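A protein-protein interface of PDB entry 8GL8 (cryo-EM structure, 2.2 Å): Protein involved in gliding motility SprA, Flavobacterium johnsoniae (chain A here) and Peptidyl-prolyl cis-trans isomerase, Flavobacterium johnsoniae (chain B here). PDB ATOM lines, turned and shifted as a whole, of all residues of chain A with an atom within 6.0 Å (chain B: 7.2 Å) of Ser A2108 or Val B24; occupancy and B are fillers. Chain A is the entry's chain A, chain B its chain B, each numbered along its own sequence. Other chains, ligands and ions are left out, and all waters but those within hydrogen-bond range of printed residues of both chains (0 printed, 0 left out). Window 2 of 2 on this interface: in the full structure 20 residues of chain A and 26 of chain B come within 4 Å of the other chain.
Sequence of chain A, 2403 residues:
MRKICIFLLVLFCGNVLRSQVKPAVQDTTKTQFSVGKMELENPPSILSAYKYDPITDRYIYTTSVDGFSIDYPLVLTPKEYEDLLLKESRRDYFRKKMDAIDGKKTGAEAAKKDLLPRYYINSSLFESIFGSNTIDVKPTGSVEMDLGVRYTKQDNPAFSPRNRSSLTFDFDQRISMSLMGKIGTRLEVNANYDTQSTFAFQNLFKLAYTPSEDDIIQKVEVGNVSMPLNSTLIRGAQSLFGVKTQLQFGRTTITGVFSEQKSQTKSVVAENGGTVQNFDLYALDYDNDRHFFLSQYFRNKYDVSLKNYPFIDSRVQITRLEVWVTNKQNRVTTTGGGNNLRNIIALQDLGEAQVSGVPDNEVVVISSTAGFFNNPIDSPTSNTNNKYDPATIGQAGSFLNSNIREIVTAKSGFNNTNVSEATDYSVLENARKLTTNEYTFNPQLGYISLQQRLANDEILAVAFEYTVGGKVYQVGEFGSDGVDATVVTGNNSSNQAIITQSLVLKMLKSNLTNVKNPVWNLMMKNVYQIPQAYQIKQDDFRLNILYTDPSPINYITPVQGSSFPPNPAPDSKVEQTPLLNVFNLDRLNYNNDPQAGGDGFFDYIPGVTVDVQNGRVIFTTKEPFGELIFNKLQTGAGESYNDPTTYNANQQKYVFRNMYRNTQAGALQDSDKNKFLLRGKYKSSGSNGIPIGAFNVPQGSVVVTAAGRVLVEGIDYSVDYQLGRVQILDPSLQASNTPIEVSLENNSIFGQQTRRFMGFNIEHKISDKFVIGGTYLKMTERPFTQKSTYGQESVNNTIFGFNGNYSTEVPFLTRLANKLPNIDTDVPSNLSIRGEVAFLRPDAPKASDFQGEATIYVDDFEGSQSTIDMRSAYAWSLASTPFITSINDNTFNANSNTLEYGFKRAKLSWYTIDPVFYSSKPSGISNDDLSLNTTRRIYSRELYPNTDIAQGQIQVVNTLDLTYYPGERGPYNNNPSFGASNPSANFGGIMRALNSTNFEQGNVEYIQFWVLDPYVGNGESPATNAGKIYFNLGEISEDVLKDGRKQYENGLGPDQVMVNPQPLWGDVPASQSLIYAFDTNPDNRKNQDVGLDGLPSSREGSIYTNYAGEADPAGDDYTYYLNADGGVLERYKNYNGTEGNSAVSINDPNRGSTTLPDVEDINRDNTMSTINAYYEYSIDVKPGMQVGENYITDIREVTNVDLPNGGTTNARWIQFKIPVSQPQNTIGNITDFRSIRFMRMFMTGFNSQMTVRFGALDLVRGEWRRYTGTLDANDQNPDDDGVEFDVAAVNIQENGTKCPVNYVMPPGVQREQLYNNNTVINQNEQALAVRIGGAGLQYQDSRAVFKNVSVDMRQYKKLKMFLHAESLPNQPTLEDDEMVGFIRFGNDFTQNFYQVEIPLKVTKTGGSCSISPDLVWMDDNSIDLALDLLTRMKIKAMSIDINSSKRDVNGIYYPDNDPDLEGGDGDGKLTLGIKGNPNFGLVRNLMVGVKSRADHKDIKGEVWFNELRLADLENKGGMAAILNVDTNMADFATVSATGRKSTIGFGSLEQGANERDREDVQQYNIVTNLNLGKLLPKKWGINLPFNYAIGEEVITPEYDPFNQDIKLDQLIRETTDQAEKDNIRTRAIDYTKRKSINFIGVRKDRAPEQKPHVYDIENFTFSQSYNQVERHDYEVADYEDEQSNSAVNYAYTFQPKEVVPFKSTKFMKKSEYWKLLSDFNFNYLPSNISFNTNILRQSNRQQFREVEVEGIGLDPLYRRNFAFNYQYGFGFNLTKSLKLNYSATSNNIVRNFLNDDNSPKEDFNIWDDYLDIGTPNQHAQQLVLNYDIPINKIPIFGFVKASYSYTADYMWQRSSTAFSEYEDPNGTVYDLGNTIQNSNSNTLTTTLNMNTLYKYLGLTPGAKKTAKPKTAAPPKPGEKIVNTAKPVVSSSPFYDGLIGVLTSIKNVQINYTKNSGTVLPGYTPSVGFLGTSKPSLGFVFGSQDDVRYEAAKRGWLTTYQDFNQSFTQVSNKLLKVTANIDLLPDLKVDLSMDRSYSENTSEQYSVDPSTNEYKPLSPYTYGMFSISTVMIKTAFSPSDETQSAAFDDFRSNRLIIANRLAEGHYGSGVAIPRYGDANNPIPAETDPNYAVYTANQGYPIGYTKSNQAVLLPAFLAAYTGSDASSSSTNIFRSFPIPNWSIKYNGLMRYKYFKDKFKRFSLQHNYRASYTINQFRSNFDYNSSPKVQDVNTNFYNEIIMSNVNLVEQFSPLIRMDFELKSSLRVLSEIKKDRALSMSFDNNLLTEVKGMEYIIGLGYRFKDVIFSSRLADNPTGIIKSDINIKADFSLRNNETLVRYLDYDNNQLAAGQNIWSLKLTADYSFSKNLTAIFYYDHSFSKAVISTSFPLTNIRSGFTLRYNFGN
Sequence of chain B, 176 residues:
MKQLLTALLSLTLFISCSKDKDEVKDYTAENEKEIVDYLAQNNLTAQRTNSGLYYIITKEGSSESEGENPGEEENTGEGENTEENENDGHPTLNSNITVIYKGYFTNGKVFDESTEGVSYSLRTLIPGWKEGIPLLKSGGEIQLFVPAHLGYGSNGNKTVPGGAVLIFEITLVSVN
Of chain B, only Val B24 (3.5 Å) comes within 4 Å of Ser A2108.
Val B24 touches three residues of chain A.
Of chain B, only Val B24, Lys B25, Asp B26 and Ser B154 come within 4 Å of Gly A2107.
Of the printed residues of chain A, Ser B154 touches Gly A2104 (3.7 Å) and Gly A2107 (3.5 Å).
Of the printed residues of chain A, Lys B25 touches Gly A2107 (2.9 Å).
Ala A2102 touches none of the printed residues of chain B.
OG of Ser B154 lies within hydrogen-bond range of O of Lys B25 (2.9 Å).
OD1 of Asp B26 sits at hydrogen-bond distance from OG1 of Thr B28.
Val B24 touches Glu A2103 (CG1 to O, 3.5 Å).
Ser B154 touches Gly A2104 (CB to O, 3.7 Å).
Gly A2107 touches Val B24 (C to CG1, 3.6 Å).
Ser B154 touches Gly A2107 (OG to CA, 3.5 Å).
CB of Ser A2108 touches CG1 of Val B24 (3.5 Å).
Gly A2109 touches Asp B26.
Of the 8 printed residues of chain B, 4 touch a printed residue of chain A.
Printed residues of chain B that touch a printed residue of chain A: Val B24, Lys B25, Asp B26 and Ser B154.
Hydrophobic or aromatic side chains of chain B within 4 Å of the printed part of chain A: Val B24.
Among the printed residues, 8 pairs touch across the chains.
The backbone carbonyl oxygen of Gly A2107 lies close to the backbone NH of Asp B26, 3.4 Å away.
The backbone carbonyl oxygen (O) of Gly A2107 sits close to the backbone carbonyl oxygen (O) of Lys B25, at 2.9 Å.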
ATOM      1  N   ALA A2102       3.848  11.715 -25.377  1.00  0.00           N
ATOM      2  CA  ALA A2102       4.043  12.843 -26.281  1.00  0.00           C
ATOM      3  C   ALA A2102       4.097  14.160 -25.519  1.00  0.00           C
ATOM      4  O   ALA A2102       4.924  15.026 -25.829  1.00  0.00           O
ATOM      5  CB  ALA A2102       2.932  12.875 -27.327  1.00  0.00           C
ATOM      6  N   GLU A2103       3.220  14.336 -24.528  1.00  0.00           N
ATOM      7  CA  GLU A2103       3.314  15.516 -23.674  1.00  0.00           C
ATOM      8  C   GLU A2103       4.648  15.550 -22.940  1.00  0.00           C
ATOM      9  O   GLU A2103       5.246  16.618 -22.772  1.00  0.00           O
ATOM     10  CB  GLU A2103       2.155  15.564 -22.678  1.00  0.00           C
ATOM     11  CG  GLU A2103       0.784  15.328 -23.283  1.00  0.00           C
ATOM     12  CD  GLU A2103      -0.190  14.702 -22.301  1.00  0.00           C
ATOM     13  OE1 GLU A2103       0.110  14.690 -21.089  1.00  0.00           O
ATOM     14  OE2 GLU A2103      -1.254  14.217 -22.742  1.00  0.00           O
ATOM     15  N   GLY A2104       5.128  14.388 -22.496  1.00  0.00           N
ATOM     16  CA  GLY A2104       6.444  14.330 -21.881  1.00  0.00           C
ATOM     17  C   GLY A2104       7.569  14.702 -22.830  1.00  0.00           C
ATOM     18  O   GLY A2104       8.569  15.288 -22.410  1.00  0.00           O
ATOM     19  N   TYR A2106       7.146  16.287 -26.336  1.00  0.00           N
ATOM     20  CA  TYR A2106       6.775  17.635 -26.757  1.00  0.00           C
ATOM     21  C   TYR A2106       6.024  18.288 -25.601  1.00  0.00           C
ATOM     22  O   TYR A2106       4.883  17.919 -25.306  1.00  0.00           O
ATOM     23  CB  TYR A2106       5.918  17.607 -28.021  1.00  0.00           C
ATOM     24  CG  TYR A2106       6.286  16.541 -29.029  1.00  0.00           C
ATOM     25  CD1 TYR A2106       7.255  16.777 -29.995  1.00  0.00           C
ATOM     26  CD2 TYR A2106       5.650  15.308 -29.030  1.00  0.00           C
ATOM     27  CE1 TYR A2106       7.588  15.810 -30.923  1.00  0.00           C
ATOM     28  CE2 TYR A2106       5.977  14.335 -29.954  1.00  0.00           C
ATOM     29  CZ  TYR A2106       6.946  14.592 -30.898  1.00  0.00           C
ATOM     30  OH  TYR A2106       7.273  13.627 -31.821  1.00  0.00           O
ATOM     31  N   GLY A2107       6.655  19.260 -24.952  1.00  0.00           N
ATOM     32  CA  GLY A2107       6.142  19.769 -23.696  1.00  0.00           C
ATOM     33  C   GLY A2107       5.086  20.853 -23.773  1.00  0.00           C
ATOM     34  O   GLY A2107       5.250  21.922 -23.179  1.00  0.00           O
ATOM     35  N   SER A2108       4.004  20.597 -24.509  1.00  0.00           N
ATOM     36  CA  SER A2108       2.785  21.404 -24.539  1.00  0.00           C
ATOM     37  C   SER A2108       2.974  22.787 -25.153  1.00  0.00           C
ATOM     38  O   SER A2108       1.991  23.524 -25.283  1.00  0.00           O
ATOM     39  CB  SER A2108       2.162  21.579 -23.147  1.00  0.00           C
ATOM     40  OG  SER A2108       2.807  22.613 -22.427  1.00  0.00           O
ATOM     41  N   GLY A2109       4.192  23.171 -25.529  1.00  0.00           N
ATOM     42  CA  GLY A2109       4.376  24.451 -26.184  1.00  0.00           C
ATOM     43  C   GLY A2109       4.046  24.459 -27.655  1.00  0.00           C
ATOM     44  O   GLY A2109       3.917  25.535 -28.248  1.00  0.00           O
ATOM     45  N   VAL A2110       3.907  23.280 -28.258  1.00  0.00           N
ATOM     46  CA  VAL A2110       3.548  23.135 -29.659  1.00  0.00           C
ATOM     47  C   VAL A2110       2.455  22.083 -29.762  1.00  0.00           C
ATOM     48  O   VAL A2110       2.245  21.278 -28.851  1.00  0.00           O
ATOM     49  CB  VAL A2110       4.754  22.742 -30.541  1.00  0.00           C
ATOM     50  CG1 VAL A2110       5.811  23.835 -30.522  1.00  0.00           C
ATOM     51  CG2 VAL A2110       5.339  21.416 -30.076  1.00  0.00           C
ATOM     52  N   ALA A2111       1.746  22.104 -30.886  1.00  0.00           N
ATOM     53  CA  ALA A2111       0.798  21.039 -31.175  1.00  0.00           C
ATOM     54  C   ALA A2111       1.555  19.738 -31.394  1.00  0.00           C
ATOM     55  O   ALA A2111       2.554  19.705 -32.119  1.00  0.00           O
ATOM     56  CB  ALA A2111      -0.039  21.387 -32.404  1.00  0.00           C
ATOM     57  N   ILE A2112       1.088  18.668 -30.761  1.00  0.00           N
ATOM     58  CA  ILE A2112       1.753  17.373 -30.862  1.00  0.00           C
ATOM     59  C   ILE A2112       1.583  16.853 -32.284  1.00  0.00           C
ATOM     60  O   ILE A2112       0.447  16.710 -32.759  1.00  0.00           O
ATOM     61  CB  ILE A2112       1.202  16.379 -29.827  1.00  0.00           C
ATOM     62  CG1 ILE A2112       1.752  16.704 -28.437  1.00  0.00           C
ATOM     63  CG2 ILE A2112       1.548  14.950 -30.215  1.00  0.00           C
ATOM     64  CD1 ILE A2112       0.970  16.073 -27.311  1.00  0.00           C
ATOM     65  N   ASP B  22       1.126  16.089 -15.756  1.00  0.00           N
ATOM     66  CA  ASP B  22       2.149  15.418 -14.964  1.00  0.00           C
ATOM     67  C   ASP B  22       3.357  16.325 -14.765  1.00  0.00           C
ATOM     68  O   ASP B  22       3.384  17.154 -13.857  1.00  0.00           O
ATOM     69  CB  ASP B  22       2.579  14.112 -15.636  1.00  0.00           C
ATOM     70  CG  ASP B  22       1.602  12.981 -15.392  1.00  0.00           C
ATOM     71  OD1 ASP B  22       1.337  12.665 -14.212  1.00  0.00           O
ATOM     72  OD2 ASP B  22       1.098  12.405 -16.380  1.00  0.00           O
ATOM     73  N   GLU B  23       4.354  16.160 -15.629  1.00  0.00           N
ATOM     74  CA  GLU B  23       5.574  16.958 -15.618  1.00  0.00           C
ATOM     75  C   GLU B  23       5.792  17.572 -16.997  1.00  0.00           C
ATOM     76  O   GLU B  23       6.875  17.515 -17.583  1.00  0.00           O
ATOM     77  CB  GLU B  23       6.765  16.107 -15.167  1.00  0.00           C
ATOM     78  CG  GLU B  23       8.077  16.863 -14.933  1.00  0.00           C
ATOM     79  CD  GLU B  23       8.110  17.631 -13.622  1.00  0.00           C
ATOM     80  OE1 GLU B  23       7.033  17.972 -13.086  1.00  0.00           O
ATOM     81  OE2 GLU B  23       9.223  17.896 -13.123  1.00  0.00           O
ATOM     82  N   VAL B  24       4.729  18.160 -17.546  1.00  0.00           N
ATOM     83  CA  VAL B  24       4.809  18.764 -18.869  1.00  0.00           C
ATOM     84  C   VAL B  24       5.442  20.143 -18.751  1.00  0.00           C
ATOM     85  O   VAL B  24       4.950  21.011 -18.019  1.00  0.00           O
ATOM     86  CB  VAL B  24       3.416  18.836 -19.510  1.00  0.00           C
ATOM     87  CG1 VAL B  24       3.536  19.152 -20.988  1.00  0.00           C
ATOM     88  CG2 VAL B  24       2.669  17.530 -19.299  1.00  0.00           C
ATOM     89  N   LYS B  25       6.537  20.351 -19.475  1.00  0.00           N
ATOM     90  CA  LYS B  25       7.331  21.568 -19.379  1.00  0.00           C
ATOM     91  C   LYS B  25       7.411  22.236 -20.743  1.00  0.00           C
ATOM     92  O   LYS B  25       7.745  21.585 -21.738  1.00  0.00           O
ATOM     93  CB  LYS B  25       8.737  21.261 -18.858  1.00  0.00           C
ATOM     94  CG  LYS B  25       8.836  21.183 -17.345  1.00  0.00           C
ATOM     95  CD  LYS B  25      10.044  20.368 -16.916  1.00  0.00           C
ATOM     96  CE  LYS B  25      10.066  19.014 -17.607  1.00  0.00           C
ATOM     97  NZ  LYS B  25      11.450  18.491 -17.772  1.00  0.00           N
ATOM     98  N   ASP B  26       7.120  23.532 -20.783  1.00  0.00           N
ATOM     99  CA  ASP B  26       7.194  24.316 -22.007  1.00  0.00           C
ATOM    100  C   ASP B  26       8.514  25.074 -22.042  1.00  0.00           C
ATOM    101  O   ASP B  26       8.849  25.792 -21.095  1.00  0.00           O
ATOM    102  CB  ASP B  26       6.018  25.289 -22.104  1.00  0.00           C
ATOM    103  CG  ASP B  26       5.922  25.955 -23.462  1.00  0.00           C
ATOM    104  OD1 ASP B  26       6.690  25.577 -24.369  1.00  0.00           O
ATOM    105  OD2 ASP B  26       5.076  26.859 -23.623  1.00  0.00           O
ATOM    106  N   TYR B  27       9.257  24.913 -23.137  1.00  0.00           N
ATOM    107  CA  TYR B  27      10.555  25.552 -23.302  1.00  0.00           C
ATOM    108  C   TYR B  27      10.609  26.464 -24.519  1.00  0.00           C
ATOM    109  O   TYR B  27      11.675  27.011 -24.819  1.00  0.00           O
ATOM    110  CB  TYR B  27      11.660  24.497 -23.410  1.00  0.00           C
ATOM    111  CG  TYR B  27      11.981  23.783 -22.120  1.00  0.00           C
ATOM    112  CD1 TYR B  27      12.770  24.382 -21.148  1.00  0.00           C
ATOM    113  CD2 TYR B  27      11.508  22.500 -21.879  1.00  0.00           C
ATOM    114  CE1 TYR B  27      13.070  23.728 -19.970  1.00  0.00           C
ATOM    115  CE2 TYR B  27      11.803  21.839 -20.706  1.00  0.00           C
ATOM    116  CZ  TYR B  27      12.584  22.457 -19.754  1.00  0.00           C
ATOM    117  OH  TYR B  27      12.880  21.799 -18.583  1.00  0.00           O
ATOM    118  N   THR B  28       9.490  26.645 -25.225  1.00  0.00           N
ATOM    119  CA  THR B  28       9.520  27.342 -26.508  1.00  0.00           C
ATOM    120  C   THR B  28       9.981  28.787 -26.351  1.00  0.00           C
ATOM    121  O   THR B  28      10.862  29.251 -27.085  1.00  0.00           O
ATOM    122  CB  THR B  28       8.140  27.285 -27.163  1.00  0.00           C
ATOM    123  OG1 THR B  28       7.127  27.403 -26.159  1.00  0.00           O
ATOM    124  CG2 THR B  28       7.959  25.972 -27.905  1.00  0.00           C
ATOM    125  N   SER B 154      11.508  17.813 -24.136  1.00  0.00           N
ATOM    126  CA  SER B 154      11.557  18.317 -22.770  1.00  0.00           C
ATOM    127  C   SER B 154      12.254  17.362 -21.811  1.00  0.00           C
ATOM    128  O   SER B 154      12.687  17.793 -20.738  1.00  0.00           O
ATOM    129  CB  SER B 154      10.141  18.603 -22.266  1.00  0.00           C
ATOM    130  OG  SER B 154       9.545  19.662 -22.993  1.00  0.00           O
